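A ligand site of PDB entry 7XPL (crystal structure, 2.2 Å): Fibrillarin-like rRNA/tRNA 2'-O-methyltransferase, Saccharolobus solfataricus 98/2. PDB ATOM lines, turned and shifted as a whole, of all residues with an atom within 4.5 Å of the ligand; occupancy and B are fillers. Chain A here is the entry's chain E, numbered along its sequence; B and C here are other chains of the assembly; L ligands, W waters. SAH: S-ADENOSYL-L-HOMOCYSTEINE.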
ATOM      1  N   ARG A  58      -7.385 -29.875  32.628  1.00  0.00           N
ATOM      2  CA  ARG A  58      -6.684 -29.997  31.366  1.00  0.00           C
ATOM      3  C   ARG A  58      -5.870 -28.758  31.011  1.00  0.00           C
ATOM      4  O   ARG A  58      -5.267 -28.726  29.925  1.00  0.00           O
ATOM      5  CB  ARG A  58      -7.675 -30.289  30.235  1.00  0.00           C
ATOM      6  CG  ARG A  58      -8.476 -31.537  30.494  1.00  0.00           C
ATOM      7  CD  ARG A  58      -9.657 -31.645  29.557  1.00  0.00           C
ATOM      8  NE  ARG A  58      -9.194 -31.678  28.179  1.00  0.00           N
ATOM      9  CZ  ARG A  58      -9.927 -32.072  27.156  1.00  0.00           C
ATOM     10  NH1 ARG A  58      -9.398 -32.052  25.939  1.00  0.00           N
ATOM     11  NH2 ARG A  58     -11.185 -32.484  27.334  1.00  0.00           N
ATOM     12  N   LYS A  60      -3.033 -25.957  32.730  1.00  0.00           N
ATOM     13  CA  LYS A  60      -2.233 -25.608  33.898  1.00  0.00           C
ATOM     14  C   LYS A  60      -2.562 -24.221  34.404  1.00  0.00           C
ATOM     15  O   LYS A  60      -2.459 -23.961  35.607  1.00  0.00           O
ATOM     16  CB  LYS A  60      -0.734 -25.672  33.565  1.00  0.00           C
ATOM     17  CG  LYS A  60      -0.286 -26.914  32.809  1.00  0.00           C
ATOM     18  CD  LYS A  60      -0.141 -28.106  33.720  1.00  0.00           C
ATOM     19  CE  LYS A  60       0.366 -29.334  32.943  1.00  0.00           C
ATOM     20  NZ  LYS A  60       0.103 -29.261  31.462  1.00  0.00           N
ATOM     21  N   TYR A  82       4.489 -18.470  23.891  1.00  0.00           N
ATOM     22  CA  TYR A  82       3.980 -19.688  24.486  1.00  0.00           C
ATOM     23  C   TYR A  82       4.843 -20.829  23.978  1.00  0.00           C
ATOM     24  O   TYR A  82       4.787 -21.185  22.794  1.00  0.00           O
ATOM     25  CB  TYR A  82       2.495 -19.879  24.137  1.00  0.00           C
ATOM     26  CG  TYR A  82       1.734 -20.903  24.950  1.00  0.00           C
ATOM     27  CD1 TYR A  82       2.221 -22.200  25.109  1.00  0.00           C
ATOM     28  CD2 TYR A  82       0.516 -20.581  25.529  1.00  0.00           C
ATOM     29  CE1 TYR A  82       1.512 -23.147  25.859  1.00  0.00           C
ATOM     30  CE2 TYR A  82      -0.201 -21.517  26.278  1.00  0.00           C
ATOM     31  CZ  TYR A  82       0.296 -22.798  26.425  1.00  0.00           C
ATOM     32  OH  TYR A  82      -0.405 -23.724  27.169  1.00  0.00           O
ATOM     33  N   GLY A  84       5.602 -24.727  24.115  1.00  0.00           N
ATOM     34  CA  GLY A  84       4.850 -25.945  24.395  1.00  0.00           C
ATOM     35  C   GLY A  84       3.364 -25.826  24.118  1.00  0.00           C
ATOM     36  O   GLY A  84       2.541 -26.229  24.942  1.00  0.00           O
ATOM     37  N   ALA A  85       3.002 -25.256  22.961  1.00  0.00           N
ATOM     38  CA  ALA A  85       1.591 -24.929  22.737  1.00  0.00           C
ATOM     39  C   ALA A  85       0.748 -26.168  22.509  1.00  0.00           C
ATOM     40  O   ALA A  85      -0.477 -26.089  22.634  1.00  0.00           O
ATOM     41  CB  ALA A  85       1.430 -24.000  21.532  1.00  0.00           C
ATOM     42  N   ALA A  86       1.355 -27.289  22.146  1.00  0.00           N
ATOM     43  CA  ALA A  86       0.678 -28.595  22.086  1.00  0.00           C
ATOM     44  C   ALA A  86      -0.466 -28.499  21.077  1.00  0.00           C
ATOM     45  O   ALA A  86      -0.272 -27.960  19.971  1.00  0.00           O
ATOM     46  CB  ALA A  86       0.270 -29.010  23.490  1.00  0.00           C
ATOM     47  N   THR A  89      -5.235 -26.486  23.741  1.00  0.00           N
ATOM     48  CA  THR A  89      -6.120 -26.341  24.877  1.00  0.00           C
ATOM     49  C   THR A  89      -5.915 -25.006  25.590  1.00  0.00           C
ATOM     50  O   THR A  89      -6.746 -24.094  25.488  1.00  0.00           O
ATOM     51  CB  THR A  89      -5.918 -27.495  25.851  1.00  0.00           C
ATOM     52  OG1 THR A  89      -6.334 -28.722  25.220  1.00  0.00           O
ATOM     53  CG2 THR A  89      -6.728 -27.285  27.122  1.00  0.00           C
ATOM     54  N   THR A  90      -4.799 -24.877  26.299  1.00  0.00           N
ATOM     55  CA  THR A  90      -4.586 -23.686  27.115  1.00  0.00           C
ATOM     56  C   THR A  90      -4.418 -22.430  26.257  1.00  0.00           C
ATOM     57  O   THR A  90      -4.996 -21.397  26.561  1.00  0.00           O
ATOM     58  CB  THR A  90      -3.396 -23.887  28.043  1.00  0.00           C
ATOM     59  OG1 THR A  90      -3.683 -24.973  28.937  1.00  0.00           O
ATOM     60  CG2 THR A  90      -3.121 -22.619  28.830  1.00  0.00           C
ATOM     61  N   VAL A 107       4.828 -21.931  20.169  1.00  0.00           N
ATOM     62  CA  VAL A 107       5.959 -22.739  19.754  1.00  0.00           C
ATOM     63  C   VAL A 107       5.686 -24.177  20.184  1.00  0.00           C
ATOM     64  O   VAL A 107       5.376 -24.427  21.352  1.00  0.00           O
ATOM     65  CB  VAL A 107       7.273 -22.212  20.371  1.00  0.00           C
ATOM     66  CG1 VAL A 107       8.464 -23.136  20.051  1.00  0.00           C
ATOM     67  CG2 VAL A 107       7.564 -20.815  19.836  1.00  0.00           C
ATOM     68  N   GLU A 108       5.822 -25.125  19.253  1.00  0.00           N
ATOM     69  CA  GLU A 108       5.602 -26.546  19.531  1.00  0.00           C
ATOM     70  C   GLU A 108       6.383 -27.360  18.505  1.00  0.00           C
ATOM     71  O   GLU A 108       6.313 -27.046  17.312  1.00  0.00           O
ATOM     72  CB  GLU A 108       4.088 -26.872  19.495  1.00  0.00           C
ATOM     73  CG  GLU A 108       3.761 -28.336  19.441  1.00  0.00           C
ATOM     74  CD  GLU A 108       4.225 -29.071  20.674  1.00  0.00           C
ATOM     75  OE1 GLU A 108       4.943 -30.092  20.549  1.00  0.00           O
ATOM     76  OE2 GLU A 108       3.892 -28.608  21.782  1.00  0.00           O
ATOM     77  N   PHE A 109       7.120 -28.391  18.951  1.00  0.00           N
ATOM     78  CA  PHE A 109       8.049 -29.047  18.019  1.00  0.00           C
ATOM     79  C   PHE A 109       7.615 -30.420  17.561  1.00  0.00           C
ATOM     80  O   PHE A 109       8.318 -31.037  16.750  1.00  0.00           O
ATOM     81  CB  PHE A 109       9.488 -29.097  18.604  1.00  0.00           C
ATOM     82  CG  PHE A 109       9.746 -30.216  19.627  1.00  0.00           C
ATOM     83  CD1 PHE A 109       8.722 -30.806  20.365  1.00  0.00           C
ATOM     84  CD2 PHE A 109      11.052 -30.644  19.855  1.00  0.00           C
ATOM     85  CE1 PHE A 109       9.005 -31.818  21.309  1.00  0.00           C
ATOM     86  CE2 PHE A 109      11.342 -31.651  20.795  1.00  0.00           C
ATOM     87  CZ  PHE A 109      10.316 -32.227  21.517  1.00  0.00           C
ATOM     88  N   SER A 110       6.488 -30.932  18.038  1.00  0.00           N
ATOM     89  CA  SER A 110       6.001 -32.243  17.628  1.00  0.00           C
ATOM     90  C   SER A 110       5.030 -32.086  16.472  1.00  0.00           C
ATOM     91  O   SER A 110       3.914 -31.599  16.674  1.00  0.00           O
ATOM     92  CB  SER A 110       5.334 -32.960  18.799  1.00  0.00           C
ATOM     93  OG  SER A 110       4.720 -34.187  18.409  1.00  0.00           O
ATOM     94  N   ALA A 132       8.507 -25.581  15.769  1.00  0.00           N
ATOM     95  CA  ALA A 132       9.858 -25.136  16.023  1.00  0.00           C
ATOM     96  C   ALA A 132      10.267 -25.727  17.353  1.00  0.00           C
ATOM     97  O   ALA A 132       9.420 -26.006  18.213  1.00  0.00           O
ATOM     98  CB  ALA A 132       9.921 -23.610  16.060  1.00  0.00           C
ATOM     99  N   ASP A 133      11.572 -25.936  17.505  1.00  0.00           N
ATOM    100  CA  ASP A 133      12.172 -26.432  18.735  1.00  0.00           C
ATOM    101  C   ASP A 133      12.486 -25.241  19.628  1.00  0.00           C
ATOM    102  O   ASP A 133      13.160 -24.310  19.196  1.00  0.00           O
ATOM    103  CB  ASP A 133      13.452 -27.214  18.405  1.00  0.00           C
ATOM    104  CG  ASP A 133      13.945 -28.031  19.555  1.00  0.00           C
ATOM    105  OD1 ASP A 133      13.746 -27.641  20.727  1.00  0.00           O
ATOM    106  OD2 ASP A 133      14.561 -29.086  19.279  1.00  0.00           O
ATOM    107  N   ALA A 134      11.972 -25.274  20.867  1.00  0.00           N
ATOM    108  CA  ALA A 134      12.218 -24.197  21.811  1.00  0.00           C
ATOM    109  C   ALA A 134      13.709 -24.038  22.152  1.00  0.00           C
ATOM    110  O   ALA A 134      14.114 -22.995  22.670  1.00  0.00           O
ATOM    111  CB  ALA A 134      11.419 -24.415  23.098  1.00  0.00           C
ATOM    112  N   ARG A 135      14.527 -25.075  21.916  1.00  0.00           N
ATOM    113  CA  ARG A 135      15.961 -24.949  22.127  1.00  0.00           C
ATOM    114  C   ARG A 135      16.618 -24.100  21.055  1.00  0.00           C
ATOM    115  O   ARG A 135      17.797 -23.761  21.208  1.00  0.00           O
ATOM    116  CB  ARG A 135      16.629 -26.342  22.179  1.00  0.00           C
ATOM    117  CG  ARG A 135      16.349 -27.090  23.499  1.00  0.00           C
ATOM    118  CD  ARG A 135      16.870 -28.557  23.519  1.00  0.00           C
ATOM    119  NE  ARG A 135      16.399 -29.290  22.351  1.00  0.00           N
ATOM    120  CZ  ARG A 135      15.520 -30.291  22.358  1.00  0.00           C
ATOM    121  NH1 ARG A 135      15.024 -30.738  23.506  1.00  0.00           N
ATOM    122  NH2 ARG A 135      15.153 -30.868  21.219  1.00  0.00           N
ATOM    123  N   ASP A 153       5.722 -24.431  29.105  1.00  0.00           N
ATOM    124  CA  ASP A 153       5.180 -25.694  29.547  1.00  0.00           C
ATOM    125  C   ASP A 153       5.728 -26.758  28.587  1.00  0.00           C
ATOM    126  O   ASP A 153       5.052 -27.257  27.708  1.00  0.00           O
ATOM    127  CB  ASP A 153       3.645 -25.679  29.588  1.00  0.00           C
ATOM    128  CG  ASP A 153       3.062 -27.000  30.124  1.00  0.00           C
ATOM    129  OD1 ASP A 153       3.839 -27.829  30.659  1.00  0.00           O
ATOM    130  OD2 ASP A 153       1.821 -27.197  30.003  1.00  0.00           O
ATOM    131  N   ILE A 154       7.020 -27.065  28.719  1.00  0.00           N
ATOM    132  CA  ILE A 154       7.651 -28.069  27.871  1.00  0.00           C
ATOM    133  C   ILE A 154       8.214 -29.173  28.746  1.00  0.00           C
ATOM    134  O   ILE A 154       8.781 -28.921  29.808  1.00  0.00           O
ATOM    135  CB  ILE A 154       8.753 -27.460  26.989  1.00  0.00           C
ATOM    136  CG1 ILE A 154       9.818 -26.794  27.872  1.00  0.00           C
ATOM    137  CG2 ILE A 154       8.121 -26.477  25.998  1.00  0.00           C
ATOM    138  CD1 ILE A 154      10.816 -25.956  27.078  1.00  0.00           C
ATOM    139  N   ALA A 155       8.004 -30.409  28.300  1.00  0.00           N
ATOM    140  CA  ALA A 155       8.587 -31.569  28.963  1.00  0.00           C
ATOM    141  C   ALA A 155      10.000 -31.757  28.415  1.00  0.00           C
ATOM    142  O   ALA A 155      10.192 -32.284  27.317  1.00  0.00           O
ATOM    143  CB  ALA A 155       7.720 -32.807  28.739  1.00  0.00           C
ATOM    144  N   GLN A 156      10.990 -31.277  29.175  1.00  0.00           N
ATOM    145  CA  GLN A 156      12.398 -31.320  28.839  1.00  0.00           C
ATOM    146  C   GLN A 156      13.147 -31.334  30.160  1.00  0.00           C
ATOM    147  O   GLN A 156      12.733 -30.622  31.090  1.00  0.00           O
ATOM    148  CB  GLN A 156      12.853 -30.126  27.994  1.00  0.00           C
ATOM    149  CG  GLN A 156      12.405 -30.148  26.553  1.00  0.00           C
ATOM    150  CD  GLN A 156      13.025 -31.302  25.776  1.00  0.00           C
ATOM    151  OE1 GLN A 156      13.981 -31.929  26.243  1.00  0.00           O
ATOM    152  NE2 GLN A 156      12.500 -31.571  24.578  1.00  0.00           N
ATOM    153  N   LYS A 182       7.733 -29.465  35.565  1.00  0.00           N
ATOM    154  CA  LYS A 182       7.240 -30.831  35.404  1.00  0.00           C
ATOM    155  C   LYS A 182       8.238 -31.779  36.049  1.00  0.00           C
ATOM    156  O   LYS A 182       9.221 -32.212  35.441  1.00  0.00           O
ATOM    157  CB  LYS A 182       7.020 -31.129  33.921  1.00  0.00           C
ATOM    158  CG  LYS A 182       6.200 -30.020  33.238  1.00  0.00           C
ATOM    159  CD  LYS A 182       6.356 -29.989  31.712  1.00  0.00           C
ATOM    160  CE  LYS A 182       5.374 -30.886  31.018  1.00  0.00           C
ATOM    161  NZ  LYS A 182       3.975 -30.683  31.524  1.00  0.00           N
ATOM    162  P     U B  18       6.935 -37.728  20.305  1.00  0.00           P
ATOM    163  OP1   U B  18       7.900 -37.272  19.297  1.00  0.00           O
ATOM    164  OP2   U B  18       7.017 -39.114  20.807  1.00  0.00           O
ATOM    165  O5'   U B  18       7.032 -36.826  21.615  1.00  0.00           O
ATOM    166  C5'   U B  18       6.951 -35.412  21.555  1.00  0.00           C
ATOM    167  C4'   U B  18       7.260 -34.816  22.899  1.00  0.00           C
ATOM    168  O4'   U B  18       6.099 -34.920  23.750  1.00  0.00           O
ATOM    169  C3'   U B  18       8.377 -35.501  23.694  1.00  0.00           C
ATOM    170  O3'   U B  18       9.663 -35.106  23.265  1.00  0.00           O
ATOM    171  C2'   U B  18       8.023 -35.121  25.139  1.00  0.00           C
ATOM    172  O2'   U B  18       8.414 -33.784  25.428  1.00  0.00           O
ATOM    173  C1'   U B  18       6.492 -35.155  25.094  1.00  0.00           C
ATOM    174  N1    U B  18       5.969 -36.478  25.502  1.00  0.00           N
ATOM    175  C2    U B  18       5.891 -36.702  26.857  1.00  0.00           C
ATOM    176  O2    U B  18       6.208 -35.841  27.636  1.00  0.00           O
ATOM    177  N3    U B  18       5.422 -37.925  27.255  1.00  0.00           N
ATOM    178  C4    U B  18       5.064 -38.951  26.423  1.00  0.00           C
ATOM    179  O4    U B  18       4.673 -40.015  26.898  1.00  0.00           O
ATOM    180  C5    U B  18       5.170 -38.657  25.034  1.00  0.00           C
ATOM    181  C6    U B  18       5.614 -37.463  24.610  1.00  0.00           C
ATOM    182  P     U C   4      -0.746 -36.195  35.773  1.00  0.00           P
ATOM    183  OP1   U C   4      -1.527 -35.337  36.701  1.00  0.00           O
ATOM    184  OP2   U C   4      -1.270 -37.555  35.417  1.00  0.00           O
ATOM    185  O5'   U C   4      -0.441 -35.386  34.428  1.00  0.00           O
ATOM    186  C5'   U C   4       0.082 -34.079  34.479  1.00  0.00           C
ATOM    187  C4'   U C   4       0.581 -33.585  33.137  1.00  0.00           C
ATOM    188  O4'   U C   4       1.720 -34.384  32.652  1.00  0.00           O
ATOM    189  C3'   U C   4      -0.399 -33.619  31.971  1.00  0.00           C
ATOM    190  O3'   U C   4      -1.368 -32.591  32.038  1.00  0.00           O
ATOM    191  C2'   U C   4       0.544 -33.553  30.764  1.00  0.00           C
ATOM    192  O2'   U C   4       1.087 -32.241  30.583  1.00  0.00           O
ATOM    193  C1'   U C   4       1.666 -34.470  31.241  1.00  0.00           C
ATOM    194  N1    U C   4       1.392 -35.879  30.850  1.00  0.00           N
ATOM    195  C2    U C   4       1.627 -36.230  29.524  1.00  0.00           C
ATOM    196  O2    U C   4       2.013 -35.443  28.683  1.00  0.00           O
ATOM    197  N3    U C   4       1.380 -37.536  29.201  1.00  0.00           N
ATOM    198  C4    U C   4       0.914 -38.526  30.063  1.00  0.00           C
ATOM    199  O4    U C   4       0.705 -39.665  29.633  1.00  0.00           O
ATOM    200  C5    U C   4       0.702 -38.087  31.411  1.00  0.00           C
ATOM    201  C6    U C   4       0.944 -36.801  31.753  1.00  0.00           C
ATOM    202  P     G C   5      -2.879 -32.871  31.573  1.00  0.00           P
ATOM    203  OP1   G C   5      -3.749 -31.818  32.145  1.00  0.00           O
ATOM    204  OP2   G C   5      -3.171 -34.318  31.847  1.00  0.00           O
ATOM    205  O5'   G C   5      -2.869 -32.733  29.985  1.00  0.00           O
ATOM    206  C5'   G C   5      -2.413 -31.547  29.354  1.00  0.00           C
ATOM    207  C4'   G C   5      -2.229 -31.737  27.870  1.00  0.00           C
ATOM    208  O4'   G C   5      -1.098 -32.621  27.603  1.00  0.00           O
ATOM    209  C3'   G C   5      -3.373 -32.388  27.124  1.00  0.00           C
ATOM    210  O3'   G C   5      -4.448 -31.507  26.867  1.00  0.00           O
ATOM    211  C2'   G C   5      -2.693 -32.909  25.877  1.00  0.00           C
ATOM    212  O2'   G C   5      -2.394 -31.858  24.981  1.00  0.00           O
ATOM    213  C1'   G C   5      -1.375 -33.405  26.455  1.00  0.00           C
ATOM    214  N9    G C   5      -1.487 -34.816  26.851  1.00  0.00           N
ATOM    215  C8    G C   5      -1.614 -35.346  28.104  1.00  0.00           C
ATOM    216  N7    G C   5      -1.719 -36.646  28.107  1.00  0.00           N
ATOM    217  C5    G C   5      -1.675 -37.004  26.765  1.00  0.00           C
ATOM    218  C6    G C   5      -1.706 -38.282  26.163  1.00  0.00           C
ATOM    219  O6    G C   5      -1.832 -39.375  26.728  1.00  0.00           O
ATOM    220  N1    G C   5      -1.619 -38.211  24.780  1.00  0.00           N
ATOM    221  C2    G C   5      -1.478 -37.021  24.082  1.00  0.00           C
ATOM    222  N2    G C   5      -1.378 -37.111  22.746  1.00  0.00           N
ATOM    223  N3    G C   5      -1.410 -35.833  24.645  1.00  0.00           N
ATOM    224  C4    G C   5      -1.526 -35.886  25.978  1.00  0.00           C
HETATM  225  N   SAH L   1       0.875 -26.388  27.314  1.00  0.00           N
HETATM  226  CA  SAH L   1      -0.107 -27.371  26.859  1.00  0.00           C
HETATM  227  CB  SAH L   1       0.385 -28.827  27.044  1.00  0.00           C
HETATM  228  CG  SAH L   1       1.895 -29.007  27.226  1.00  0.00           C
HETATM  229  SD  SAH L   1       2.370 -30.756  26.977  1.00  0.00           S
HETATM  230  C   SAH L   1      -1.502 -27.172  27.482  1.00  0.00           C
HETATM  231  O   SAH L   1      -2.510 -27.387  26.808  1.00  0.00           O
HETATM  232  OXT SAH L   1      -1.639 -26.799  28.654  1.00  0.00           O
HETATM  233  C5' SAH L   1       4.152 -30.363  26.744  1.00  0.00           C
HETATM  234  C4' SAH L   1       4.458 -29.999  25.303  1.00  0.00           C
HETATM  235  O4' SAH L   1       5.743 -29.406  25.170  1.00  0.00           O
HETATM  236  C3' SAH L   1       4.447 -31.211  24.367  1.00  0.00           C
HETATM  237  O3' SAH L   1       3.599 -30.942  23.282  1.00  0.00           O
HETATM  238  C2' SAH L   1       5.841 -31.257  23.792  1.00  0.00           C
HETATM  239  O2' SAH L   1       5.803 -31.615  22.429  1.00  0.00           O
HETATM  240  C1' SAH L   1       6.274 -29.815  23.934  1.00  0.00           C
HETATM  241  N9  SAH L   1       7.748 -29.691  23.881  1.00  0.00           N
HETATM  242  C8  SAH L   1       8.668 -30.428  24.584  1.00  0.00           C
HETATM  243  N7  SAH L   1       9.898 -30.014  24.249  1.00  0.00           N
HETATM  244  C5  SAH L   1       9.771 -29.038  23.322  1.00  0.00           C
HETATM  245  C6  SAH L   1      10.707 -28.278  22.636  1.00  0.00           C
HETATM  246  N6  SAH L   1      11.998 -28.481  22.870  1.00  0.00           N
HETATM  247  N1  SAH L   1      10.286 -27.319  21.737  1.00  0.00           N
HETATM  248  C2  SAH L   1       8.929 -27.119  21.523  1.00  0.00           C
HETATM  249  N3  SAH L   1       7.995 -27.885  22.202  1.00  0.00           N
HETATM  250  C4  SAH L   1       8.426 -28.829  23.089  1.00  0.00           C
HETATM  251  O   HOH W   1      -0.049 -25.094  29.909  1.00  0.00           O
HETATM  252  O   HOH W   2      -2.262 -24.843  24.544  1.00  0.00           O
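Water W1 lies within hydrogen-bond range of OXT of the ligand (2.6 Å), OD2 of Asp 153 (2.8 Å) and OH of Tyr 82 (3.1 Å). Water W2 lies within hydrogen-bond range of O of Ala 85, N of Thr 90, OH of Tyr 82, O of the ligand and N of Thr 89.
The backbone carbonyl oxygen of Glu 108 lies within hydrogen-bond range of the backbone NH of Ala 132. The backbone NH (N) of Ala 86 is in hydrogen-bond range of the side-chain carboxylate (OE2) of Glu 108. The side-chain carboxylate (OE1) of Glu 108 sits at hydrogen-bond distance from the backbone NH (N) of Ser 110, at 3.1 Å. The side-chain carboxylate of Asp 133 lies within salt-bridge range of the guanidinium group of Arg 135 (2.7 Å). N of Gly 84 is in hydrogen-bond range of O of Val 107, at 2.8 Å. The side-chain carboxylate (OD2) of Asp 153 lies within salt-bridge range of the side-chain amino group (NZ) of Lys 60, 3.1 Å away. The side-chain amino group (NZ) of Lys 182 lies within salt-bridge range of the side-chain carboxylate (OD1) of Asp 153 (3.0 Å). The side-chain amide nitrogen (NE2) of Gln 156 lies close to the guanidinium group (NH1) of Arg 135 (2.9 Å).
OE1 of Glu 108 sits at hydrogen-bond distance from O2' of the ligand (2.6 Å). O of the ligand sits at hydrogen-bond distance from N of Thr 90 (3.4 Å). The side-chain hydroxyl of Thr 90 sits at hydrogen-bond distance from an oxygen (OXT) of the ligand (2.8 Å). The backbone NH (N) of Ala 134 is in hydrogen-bond range of a nitrogen (N1) of the ligand. N6 of the ligand sits at hydrogen-bond distance from OD1 of Asp 133. O of Gly 84 is in hydrogen-bond range of N of the ligand (2.9 Å). A nitrogen (N) of the ligand sits at hydrogen-bond distance from the side-chain hydroxyl (OH) of Tyr 82 (3.0 Å). OD2 of Asp 153 is in salt-bridge range of N of the ligand, at 3.0 Å. The side-chain amide nitrogen (NE2) of Gln 156 lies within hydrogen-bond range of a nitrogen (N7) of the ligand, 3.1 Å away. N of Phe 109 lies close to N3 of the ligand (3.4 Å).
Merely in contact with the ligand: Ala 86 (3.6 Å), Thr 89 (3.5 Å), Ser 110 (3.9 Å), Ala 132 (3.5 Å), Arg 135 (3.8 Å), Ile 154 (3.6 Å), Ala 155 (3.6 Å), U 18 of chain B (3.5 Å) and G 5 of chain C (3.99 Å). Hydrophobic or aromatic side chains within 4 Å of the ligand: Tyr 82, Ala 86, Phe 109, Ala 134 and Ile 154. 18 residues have an atom within 4 Å of the ligand: Tyr 82, Gly 84, Ala 86, Thr 89, Thr 90, Glu 108, Phe 109, Ser 110, Ala 132, Asp 133, Ala 134, Arg 135, Asp 153, Ile 154, Ala 155, Gln 156, U 18 of chain B and G 5 of chain C. The nearest printed residue that does not touch the ligand is U 4 of chain C (4.1 Å).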
